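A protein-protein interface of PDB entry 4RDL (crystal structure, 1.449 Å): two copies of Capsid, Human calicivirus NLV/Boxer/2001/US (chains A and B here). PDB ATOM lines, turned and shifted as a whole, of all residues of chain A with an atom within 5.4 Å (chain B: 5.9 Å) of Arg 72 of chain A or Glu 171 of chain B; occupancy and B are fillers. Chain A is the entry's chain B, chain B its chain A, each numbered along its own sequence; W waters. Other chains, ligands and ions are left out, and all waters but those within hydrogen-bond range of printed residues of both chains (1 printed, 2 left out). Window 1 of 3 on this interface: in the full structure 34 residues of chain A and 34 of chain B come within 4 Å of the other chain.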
ATOM      1  N   ALA A  68      24.744   5.988  -8.421  1.00  0.00           N
ATOM      2  CA  ALA A  68      23.544   5.815  -9.240  1.00  0.00           C
ATOM      3  C   ALA A  68      22.362   6.668  -8.769  1.00  0.00           C
ATOM      4  O   ALA A  68      21.387   6.844  -9.506  1.00  0.00           O
ATOM      5  CB  ALA A  68      23.141   4.334  -9.314  1.00  0.00           C
ATOM      6  N   CYS A  69      22.444   7.197  -7.552  1.00  0.00           N
ATOM      7  CA  CYS A  69      21.347   8.004  -6.999  1.00  0.00           C
ATOM      8  C   CYS A  69      21.551   9.509  -7.138  1.00  0.00           C
ATOM      9  O   CYS A  69      20.637  10.288  -6.874  1.00  0.00           O
ATOM     10  CB  CYS A  69      21.152   7.696  -5.521  1.00  0.00           C
ATOM     11  SG  CYS A  69      20.745   5.984  -5.182  1.00  0.00           S
ATOM     12  N   ILE A  70      22.755   9.923  -7.520  1.00  0.00           N
ATOM     13  CA  ILE A  70      23.107  11.339  -7.481  1.00  0.00           C
ATOM     14  C   ILE A  70      22.274  12.193  -8.442  1.00  0.00           C
ATOM     15  O   ILE A  70      22.204  11.914  -9.644  1.00  0.00           O
ATOM     16  CB  ILE A  70      24.596  11.560  -7.781  1.00  0.00           C
ATOM     17  CG1 ILE A  70      25.489  10.868  -6.742  1.00  0.00           C
ATOM     18  CG2 ILE A  70      24.902  13.051  -7.814  1.00  0.00           C
ATOM     19  CD1 ILE A  70      26.947  10.808  -7.158  1.00  0.00           C
ATOM     20  N   ALA A  71      21.647  13.228  -7.885  1.00  0.00           N
ATOM     21  CA  ALA A  71      20.907  14.241  -8.645  1.00  0.00           C
ATOM     22  C   ALA A  71      19.703  13.659  -9.376  1.00  0.00           C
ATOM     23  O   ALA A  71      19.377  14.061 -10.487  1.00  0.00           O
ATOM     24  CB  ALA A  71      21.830  15.010  -9.610  1.00  0.00           C
ATOM     25  N   ARG A  72      19.033  12.718  -8.722  1.00  0.00           N
ATOM     26  CA  ARG A  72      17.829  12.106  -9.259  1.00  0.00           C
ATOM     27  C   ARG A  72      16.643  12.358  -8.346  1.00  0.00           C
ATOM     28  O   ARG A  72      16.812  12.723  -7.178  1.00  0.00           O
ATOM     29  CB  ARG A  72      18.049  10.606  -9.480  1.00  0.00           C
ATOM     30  CG  ARG A  72      19.083  10.343 -10.560  1.00  0.00           C
ATOM     31  CD  ARG A  72      19.256   8.860 -10.823  1.00  0.00           C
ATOM     32  NE  ARG A  72      20.308   8.600 -11.794  1.00  0.00           N
ATOM     33  CZ  ARG A  72      20.098   8.215 -13.051  1.00  0.00           C
ATOM     34  NH1 ARG A  72      18.861   8.046 -13.501  1.00  0.00           N
ATOM     35  NH2 ARG A  72      21.129   7.990 -13.861  1.00  0.00           N
ATOM     36  N   MET A  73      15.446  12.184  -8.899  1.00  0.00           N
ATOM     37  CA  MET A  73      14.204  12.312  -8.150  1.00  0.00           C
ATOM     38  C   MET A  73      13.270  11.193  -8.558  1.00  0.00           C
ATOM     39  O   MET A  73      13.427  10.603  -9.624  1.00  0.00           O
ATOM     40  CB  MET A  73      13.496  13.635  -8.465  1.00  0.00           C
ATOM     41  CG  MET A  73      14.334  14.888  -8.336  1.00  0.00           C
ATOM     42  SD  MET A  73      13.347  16.288  -8.893  1.00  0.00           S
ATOM     43  CE  MET A  73      14.573  17.603  -8.862  1.00  0.00           C
ATOM     44  N   ARG A  74      12.271  10.930  -7.720  1.00  0.00           N
ATOM     45  CA  ARG A  74      11.220   9.984  -8.074  1.00  0.00           C
ATOM     46  C   ARG A  74       9.905  10.461  -7.498  1.00  0.00           C
ATOM     47  O   ARG A  74       9.872  11.052  -6.416  1.00  0.00           O
ATOM     48  CB  ARG A  74      11.537   8.588  -7.538  1.00  0.00           C
ATOM     49  CG  ARG A  74      10.454   7.554  -7.843  1.00  0.00           C
ATOM     50  CD  ARG A  74      10.945   6.145  -7.538  1.00  0.00           C
ATOM     51  NE  ARG A  74       9.918   5.142  -7.806  1.00  0.00           N
ATOM     52  CZ  ARG A  74      10.177   3.867  -8.062  1.00  0.00           C
ATOM     53  NH1 ARG A  74      11.433   3.439  -8.087  1.00  0.00           N
ATOM     54  NH2 ARG A  74       9.185   3.018  -8.284  1.00  0.00           N
ATOM     55  N   LEU A  91      14.050   7.079  -4.112  1.00  0.00           N
ATOM     56  CA  LEU A  91      14.352   6.558  -5.451  1.00  0.00           C
ATOM     57  C   LEU A  91      13.956   5.099  -5.668  1.00  0.00           C
ATOM     58  O   LEU A  91      13.753   4.673  -6.803  1.00  0.00           O
ATOM     59  CB  LEU A  91      15.833   6.762  -5.795  1.00  0.00           C
ATOM     60  CG  LEU A  91      16.232   8.228  -5.960  1.00  0.00           C
ATOM     61  CD1 LEU A  91      17.740   8.344  -6.168  1.00  0.00           C
ATOM     62  CD2 LEU A  91      15.490   8.883  -7.126  1.00  0.00           C
ATOM     63  N   LEU A 105      16.660  10.988  -0.568  1.00  0.00           N
ATOM     64  CA  LEU A 105      18.080  10.761  -0.825  1.00  0.00           C
ATOM     65  C   LEU A 105      18.394  10.908  -2.318  1.00  0.00           C
ATOM     66  O   LEU A 105      17.598  10.494  -3.172  1.00  0.00           O
ATOM     67  CB  LEU A 105      18.522   9.388  -0.307  1.00  0.00           C
ATOM     68  CG  LEU A 105      18.283   9.148   1.185  1.00  0.00           C
ATOM     69  CD1 LEU A 105      18.894   7.811   1.580  1.00  0.00           C
ATOM     70  CD2 LEU A 105      18.864  10.287   2.031  1.00  0.00           C
ATOM     71  N   GLY A 106      19.538  11.531  -2.619  1.00  0.00           N
ATOM     72  CA  GLY A 106      19.988  11.722  -3.989  1.00  0.00           C
ATOM     73  C   GLY A 106      19.503  13.014  -4.633  1.00  0.00           C
ATOM     74  O   GLY A 106      20.008  13.414  -5.683  1.00  0.00           O
ATOM     75  N   PHE A 107      18.532  13.675  -4.013  1.00  0.00           N
ATOM     76  CA  PHE A 107      17.913  14.860  -4.597  1.00  0.00           C
ATOM     77  C   PHE A 107      18.983  15.891  -4.975  1.00  0.00           C
ATOM     78  O   PHE A 107      19.919  16.114  -4.215  1.00  0.00           O
ATOM     79  CB  PHE A 107      16.935  15.473  -3.589  1.00  0.00           C
ATOM     80  CG  PHE A 107      15.887  16.358  -4.208  1.00  0.00           C
ATOM     81  CD1 PHE A 107      14.690  15.825  -4.669  1.00  0.00           C
ATOM     82  CD2 PHE A 107      16.093  17.725  -4.314  1.00  0.00           C
ATOM     83  CE1 PHE A 107      13.723  16.645  -5.233  1.00  0.00           C
ATOM     84  CE2 PHE A 107      15.134  18.544  -4.880  1.00  0.00           C
ATOM     85  CZ  PHE A 107      13.948  18.003  -5.336  1.00  0.00           C
ATOM     86  N   PRO A 108      18.850  16.527  -6.152  1.00  0.00           N
ATOM     87  CA  PRO A 108      19.855  17.544  -6.512  1.00  0.00           C
ATOM     88  C   PRO A 108      20.002  18.632  -5.439  1.00  0.00           C
ATOM     89  O   PRO A 108      19.003  19.049  -4.852  1.00  0.00           O
ATOM     90  CB  PRO A 108      19.300  18.157  -7.809  1.00  0.00           C
ATOM     91  CG  PRO A 108      18.378  17.130  -8.371  1.00  0.00           C
ATOM     92  CD  PRO A 108      17.827  16.344  -7.195  1.00  0.00           C
ATOM     93  N   MET A 117      15.351  18.460 -16.234  1.00  0.00           N
ATOM     94  CA  MET A 117      15.287  17.030 -15.969  1.00  0.00           C
ATOM     95  C   MET A 117      14.848  16.228 -17.185  1.00  0.00           C
ATOM     96  O   MET A 117      14.031  16.681 -17.990  1.00  0.00           O
ATOM     97  CB  MET A 117      14.308  16.739 -14.826  1.00  0.00           C
ATOM     98  CG  MET A 117      14.453  17.637 -13.597  1.00  0.00           C
ATOM     99  SD  MET A 117      16.021  17.468 -12.728  1.00  0.00           S
ATOM    100  CE  MET A 117      15.859  15.814 -12.025  1.00  0.00           C
ATOM    101  N   LEU A 170      13.274  10.832 -12.370  1.00  0.00           N
ATOM    102  CA  LEU A 170      13.853  11.983 -13.057  1.00  0.00           C
ATOM    103  C   LEU A 170      15.353  12.055 -12.795  1.00  0.00           C
ATOM    104  O   LEU A 170      15.822  11.727 -11.701  1.00  0.00           O
ATOM    105  CB  LEU A 170      13.198  13.278 -12.576  1.00  0.00           C
ATOM    106  CG  LEU A 170      11.670  13.368 -12.649  1.00  0.00           C
ATOM    107  CD1 LEU A 170      11.050  13.064 -11.279  1.00  0.00           C
ATOM    108  CD2 LEU A 170      11.236  14.741 -13.149  1.00  0.00           C
ATOM    109  N   GLU A 171      16.099  12.511 -13.792  1.00  0.00           N
ATOM    110  CA  GLU A 171      17.535  12.717 -13.647  1.00  0.00           C
ATOM    111  C   GLU A 171      17.904  14.105 -14.156  1.00  0.00           C
ATOM    112  O   GLU A 171      17.273  14.643 -15.072  1.00  0.00           O
ATOM    113  CB  GLU A 171      18.321  11.633 -14.387  1.00  0.00           C
ATOM    114  CG  GLU A 171      18.010  11.548 -15.868  1.00  0.00           C
ATOM    115  CD  GLU A 171      18.903  10.579 -16.621  1.00  0.00           C
ATOM    116  OE1 GLU A 171      19.989  10.242 -16.106  1.00  0.00           O
ATOM    117  OE2 GLU A 171      18.512  10.153 -17.732  1.00  0.00           O
ATOM    118  N   LEU A 172      18.939  14.680 -13.562  1.00  0.00           N
ATOM    119  CA  LEU A 172      19.380  16.019 -13.930  1.00  0.00           C
ATOM    120  C   LEU A 172      20.214  15.993 -15.206  1.00  0.00           C
ATOM    121  O   LEU A 172      21.344  15.513 -15.216  1.00  0.00           O
ATOM    122  CB  LEU A 172      20.191  16.624 -12.784  1.00  0.00           C
ATOM    123  CG  LEU A 172      20.646  18.072 -12.970  1.00  0.00           C
ATOM    124  CD1 LEU A 172      19.440  19.001 -13.089  1.00  0.00           C
ATOM    125  CD2 LEU A 172      21.551  18.491 -11.816  1.00  0.00           C
ATOM    126  N   PRO B  30      22.635   2.516 -14.495  1.00  0.00           N
ATOM    127  CA  PRO B  30      22.811   3.178 -13.198  1.00  0.00           C
ATOM    128  C   PRO B  30      21.475   3.272 -12.461  1.00  0.00           C
ATOM    129  O   PRO B  30      20.783   4.295 -12.503  1.00  0.00           O
ATOM    130  CB  PRO B  30      23.358   4.553 -13.587  1.00  0.00           C
ATOM    131  CG  PRO B  30      22.723   4.811 -14.915  1.00  0.00           C
ATOM    132  CD  PRO B  30      22.692   3.474 -15.619  1.00  0.00           C
ATOM    133  N   MET B  31      21.114   2.173 -11.802  1.00  0.00           N
ATOM    134  CA  MET B  31      19.858   2.048 -11.076  1.00  0.00           C
ATOM    135  C   MET B  31      20.113   1.195  -9.861  1.00  0.00           C
ATOM    136  O   MET B  31      20.871   0.229  -9.929  1.00  0.00           O
ATOM    137  CB  MET B  31      18.798   1.331 -11.917  1.00  0.00           C
ATOM    138  CG  MET B  31      18.374   2.023 -13.182  1.00  0.00           C
ATOM    139  SD  MET B  31      17.571   3.598 -12.876  1.00  0.00           S
ATOM    140  CE  MET B  31      16.369   3.185 -11.644  1.00  0.00           C
ATOM    141  N   ILE B  70      28.339   4.036 -16.143  1.00  0.00           N
ATOM    142  CA  ILE B  70      27.566   2.937 -16.698  1.00  0.00           C
ATOM    143  C   ILE B  70      26.588   3.374 -17.787  1.00  0.00           C
ATOM    144  O   ILE B  70      25.780   4.287 -17.581  1.00  0.00           O
ATOM    145  CB  ILE B  70      26.796   2.193 -15.590  1.00  0.00           C
ATOM    146  CG1 ILE B  70      27.766   1.606 -14.558  1.00  0.00           C
ATOM    147  CG2 ILE B  70      25.915   1.094 -16.192  1.00  0.00           C
ATOM    148  CD1 ILE B  70      27.060   1.136 -13.296  1.00  0.00           C
ATOM    149  N   ALA B  71      26.686   2.713 -18.943  1.00  0.00           N
ATOM    150  CA  ALA B  71      25.759   2.904 -20.057  1.00  0.00           C
ATOM    151  C   ALA B  71      25.810   4.314 -20.627  1.00  0.00           C
ATOM    152  O   ALA B  71      24.801   4.863 -21.057  1.00  0.00           O
ATOM    153  CB  ALA B  71      24.330   2.514 -19.654  1.00  0.00           C
ATOM    154  N   ARG B  72      27.006   4.887 -20.633  1.00  0.00           N
ATOM    155  CA  ARG B  72      27.231   6.200 -21.224  1.00  0.00           C
ATOM    156  C   ARG B  72      28.183   6.098 -22.401  1.00  0.00           C
ATOM    157  O   ARG B  72      28.872   5.086 -22.561  1.00  0.00           O
ATOM    158  CB  ARG B  72      27.766   7.175 -20.173  1.00  0.00           C
ATOM    159  CG  ARG B  72      26.736   7.484 -19.089  1.00  0.00           C
ATOM    160  CD  ARG B  72      27.238   8.495 -18.078  1.00  0.00           C
ATOM    161  NE  ARG B  72      26.307   8.645 -16.963  1.00  0.00           N
ATOM    162  CZ  ARG B  72      25.535   9.710 -16.761  1.00  0.00           C
ATOM    163  NH1 ARG B  72      25.567  10.730 -17.607  1.00  0.00           N
ATOM    164  NH2 ARG B  72      24.728   9.754 -15.704  1.00  0.00           N
ATOM    165  N   MET B  73      28.194   7.146 -23.221  1.00  0.00           N
ATOM    166  CA  MET B  73      29.126   7.281 -24.335  1.00  0.00           C
ATOM    167  C   MET B  73      29.640   8.706 -24.375  1.00  0.00           C
ATOM    168  O   MET B  73      29.037   9.620 -23.802  1.00  0.00           O
ATOM    169  CB  MET B  73      28.440   6.995 -25.671  1.00  0.00           C
ATOM    170  CG  MET B  73      27.664   5.691 -25.747  1.00  0.00           C
ATOM    171  SD  MET B  73      26.798   5.649 -27.343  1.00  0.00           S
ATOM    172  CE  MET B  73      25.776   4.190 -27.150  1.00  0.00           C
ATOM    173  N   HIS B 116      17.987   4.566 -26.831  1.00  0.00           N
ATOM    174  CA  HIS B 116      17.471   5.929 -26.852  1.00  0.00           C
ATOM    175  C   HIS B 116      18.297   6.756 -25.892  1.00  0.00           C
ATOM    176  O   HIS B 116      18.182   6.607 -24.669  1.00  0.00           O
ATOM    177  CB  HIS B 116      15.990   5.947 -26.467  1.00  0.00           C
ATOM    178  CG  HIS B 116      15.135   5.140 -27.391  1.00  0.00           C
ATOM    179  ND1 HIS B 116      14.480   5.696 -28.471  1.00  0.00           N
ATOM    180  CD2 HIS B 116      14.870   3.813 -27.429  1.00  0.00           C
ATOM    181  CE1 HIS B 116      13.826   4.747 -29.119  1.00  0.00           C
ATOM    182  NE2 HIS B 116      14.055   3.594 -28.513  1.00  0.00           N
ATOM    183  N   MET B 117      19.144   7.611 -26.459  1.00  0.00           N
ATOM    184  CA  MET B 117      20.134   8.350 -25.687  1.00  0.00           C
ATOM    185  C   MET B 117      19.705   9.787 -25.479  1.00  0.00           C
ATOM    186  O   MET B 117      19.097  10.411 -26.356  1.00  0.00           O
ATOM    187  CB  MET B 117      21.491   8.353 -26.403  1.00  0.00           C
ATOM    188  CG  MET B 117      21.978   6.992 -26.883  1.00  0.00           C
ATOM    189  SD  MET B 117      22.304   5.807 -25.568  1.00  0.00           S
ATOM    190  CE  MET B 117      23.752   6.500 -24.789  1.00  0.00           C
ATOM    191  N   THR B 118      20.053  10.322 -24.320  1.00  0.00           N
ATOM    192  CA  THR B 118      19.978  11.751 -24.092  1.00  0.00           C
ATOM    193  C   THR B 118      21.414  12.254 -24.086  1.00  0.00           C
ATOM    194  O   THR B 118      22.303  11.570 -23.587  1.00  0.00           O
ATOM    195  CB  THR B 118      19.282  12.053 -22.764  1.00  0.00           C
ATOM    196  OG1 THR B 118      17.891  11.727 -22.883  1.00  0.00           O
ATOM    197  CG2 THR B 118      19.417  13.524 -22.397  1.00  0.00           C
ATOM    198  N   PHE B 119      21.668  13.431 -24.648  1.00  0.00           N
ATOM    199  CA  PHE B 119      23.039  13.920 -24.672  1.00  0.00           C
ATOM    200  C   PHE B 119      23.156  15.409 -24.404  1.00  0.00           C
ATOM    201  O   PHE B 119      22.190  16.166 -24.548  1.00  0.00           O
ATOM    202  CB  PHE B 119      23.757  13.549 -25.979  1.00  0.00           C
ATOM    203  CG  PHE B 119      23.207  14.231 -27.208  1.00  0.00           C
ATOM    204  CD1 PHE B 119      23.611  15.518 -27.553  1.00  0.00           C
ATOM    205  CD2 PHE B 119      22.301  13.577 -28.030  1.00  0.00           C
ATOM    206  CE1 PHE B 119      23.113  16.133 -28.688  1.00  0.00           C
ATOM    207  CE2 PHE B 119      21.809  14.184 -29.171  1.00  0.00           C
ATOM    208  CZ  PHE B 119      22.212  15.462 -29.495  1.00  0.00           C
ATOM    209  N   VAL B 169      28.482  14.156 -24.415  1.00  0.00           N
ATOM    210  CA  VAL B 169      28.349  12.947 -23.615  1.00  0.00           C
ATOM    211  C   VAL B 169      26.908  12.467 -23.715  1.00  0.00           C
ATOM    212  O   VAL B 169      25.961  13.272 -23.694  1.00  0.00           O
ATOM    213  CB  VAL B 169      28.781  13.165 -22.152  1.00  0.00           C
ATOM    214  CG1 VAL B 169      30.283  13.361 -22.070  1.00  0.00           C
ATOM    215  CG2 VAL B 169      28.063  14.332 -21.532  1.00  0.00           C
ATOM    216  N   LEU B 170      26.752  11.157 -23.881  1.00  0.00           N
ATOM    217  CA  LEU B 170      25.444  10.547 -24.078  1.00  0.00           C
ATOM    218  C   LEU B 170      25.153   9.595 -22.934  1.00  0.00           C
ATOM    219  O   LEU B 170      26.055   8.928 -22.420  1.00  0.00           O
ATOM    220  CB  LEU B 170      25.403   9.787 -25.404  1.00  0.00           C
ATOM    221  CG  LEU B 170      25.794  10.577 -26.664  1.00  0.00           C
ATOM    222  CD1 LEU B 170      27.211  10.215 -27.104  1.00  0.00           C
ATOM    223  CD2 LEU B 170      24.805  10.281 -27.769  1.00  0.00           C
ATOM    224  N   GLU B 171      23.887   9.543 -22.531  1.00  0.00           N
ATOM    225  CA  GLU B 171      23.459   8.617 -21.494  1.00  0.00           C
ATOM    226  C   GLU B 171      22.263   7.816 -21.986  1.00  0.00           C
ATOM    227  O   GLU B 171      21.424   8.318 -22.734  1.00  0.00           O
ATOM    228  CB  GLU B 171      23.100   9.349 -20.207  1.00  0.00           C
ATOM    229  CG  GLU B 171      22.934   8.380 -19.043  1.00  0.00           C
ATOM    230  CD  GLU B 171      22.192   8.971 -17.871  1.00  0.00           C
ATOM    231  OE1 GLU B 171      21.888   8.198 -16.931  1.00  0.00           O
ATOM    232  OE2 GLU B 171      21.923  10.196 -17.886  1.00  0.00           O
ATOM    233  N   LEU B 172      22.189   6.563 -21.562  1.00  0.00           N
ATOM    234  CA  LEU B 172      21.103   5.686 -21.963  1.00  0.00           C
ATOM    235  C   LEU B 172      19.827   6.015 -21.194  1.00  0.00           C
ATOM    236  O   LEU B 172      19.728   5.758 -19.996  1.00  0.00           O
ATOM    237  CB  LEU B 172      21.506   4.229 -21.729  1.00  0.00           C
ATOM    238  CG  LEU B 172      20.480   3.204 -22.217  1.00  0.00           C
ATOM    239  CD1 LEU B 172      20.279   3.307 -23.731  1.00  0.00           C
ATOM    240  CD2 LEU B 172      20.920   1.798 -21.822  1.00  0.00           C
ATOM    241  N   THR B 173      18.841   6.579 -21.882  1.00  0.00           N
ATOM    242  CA  THR B 173      17.585   6.959 -21.229  1.00  0.00           C
ATOM    243  C   THR B 173      16.593   5.802 -21.202  1.00  0.00           C
ATOM    244  O   THR B 173      15.973   5.523 -20.170  1.00  0.00           O
ATOM    245  CB  THR B 173      16.954   8.177 -21.915  1.00  0.00           C
ATOM    246  OG1 THR B 173      17.899   9.251 -21.870  1.00  0.00           O
ATOM    247  CG2 THR B 173      15.668   8.612 -21.218  1.00  0.00           C
HETATM  248  O   HOH W   1      22.014  11.093 -14.655  1.00  0.00           O
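Of the 16 printed residues of chain A, 3 touch a printed residue of chain B.
Hydrophobic or aromatic side chains of chain A within 4 Å of the printed part of chain B: Ala 68.
Hydrophobic or aromatic side chains of chain B that line the printed part of chain A: Pro 30.
Among the printed residues, Asp or Glu carboxylates within 4 Å of a Lys or Arg side-chain nitrogen of the other chain: Arg 72 of chain A with Glu 171 of chain B (3.2 Å).
Water W1 lies within hydrogen-bond range of the side-chain carboxylate of Glu 171 of chain A (2.6 Å), the guanidinium group of Arg 72 of chain B (3.2 Å), the guanidinium group of Arg 72 of chain A (3.3 Å) and the side-chain carboxylate of Glu 171 of chain B (3.4 Å).
OE1 of Glu 171 of chain B is in salt-bridge range of NH2 of Arg 72 of chain A, 3.2 Å away.
OE2 of Glu 171 of chain B sits close to OE1 of Glu 171 of chain A.
Arg 72 of chain A touches Glu 171 of chain B, but with the chains exchanged Glu 171 of chain A does not touch Arg 72 of chain B (4.8 Å).
Glu 171 of chain B touches its own counterpart, Glu 171 of chain A.
Of the printed residues of chain B, Ala 68 of chain A touches Pro 30 and Met 31.
Arg 72 of chain A touches just these residues of chain B: Pro 30 and Glu 171.
Printed residues of chain B within 4 Å of Glu 171 of chain A: Glu 171 (2.6 Å).
Of the printed residues of chain A, Pro 30 of chain B touches Ala 68 and Arg 72.
Of the printed residues of chain A, Met 31 of chain B touches Ala 68.
Leu 170 of chain B touches none of the printed residues of chain A.
Of the printed residues of chain A, Glu 171 of chain B touches Arg 72 (3.2 Å) and Glu 171 (2.6 Å).
CB of Ala 68 of chain A touches C of Pro 30 of chain B, at 3.7 Å.
Ala 68 of chain A touches Met 31 of chain B.
CG of Pro 30 of chain B touches NH2 of Arg 72 of chain A, at 3.7 Å.
NH2 of Arg 72 of chain B is in salt-bridge range of OE1 of Glu 171 of chain B (3.5 Å).
The backbone carbonyl oxygen (O) of Thr 118 of chain B lies within hydrogen-bond range of the backbone NH (N) of Glu 171 of chain B (2.8 Å).
O of Ala 68 of chain A sits at hydrogen-bond distance from NE of Arg 72 of chain A.
N of Arg 72 of chain A sits at hydrogen-bond distance from O of Gly 106 of chain A (3.3 Å).
The side-chain carboxylate (OE1) of Glu 171 of chain A lies within salt-bridge range of the guanidinium group (NH2) of Arg 72 of chain A, 3.4 Å away.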
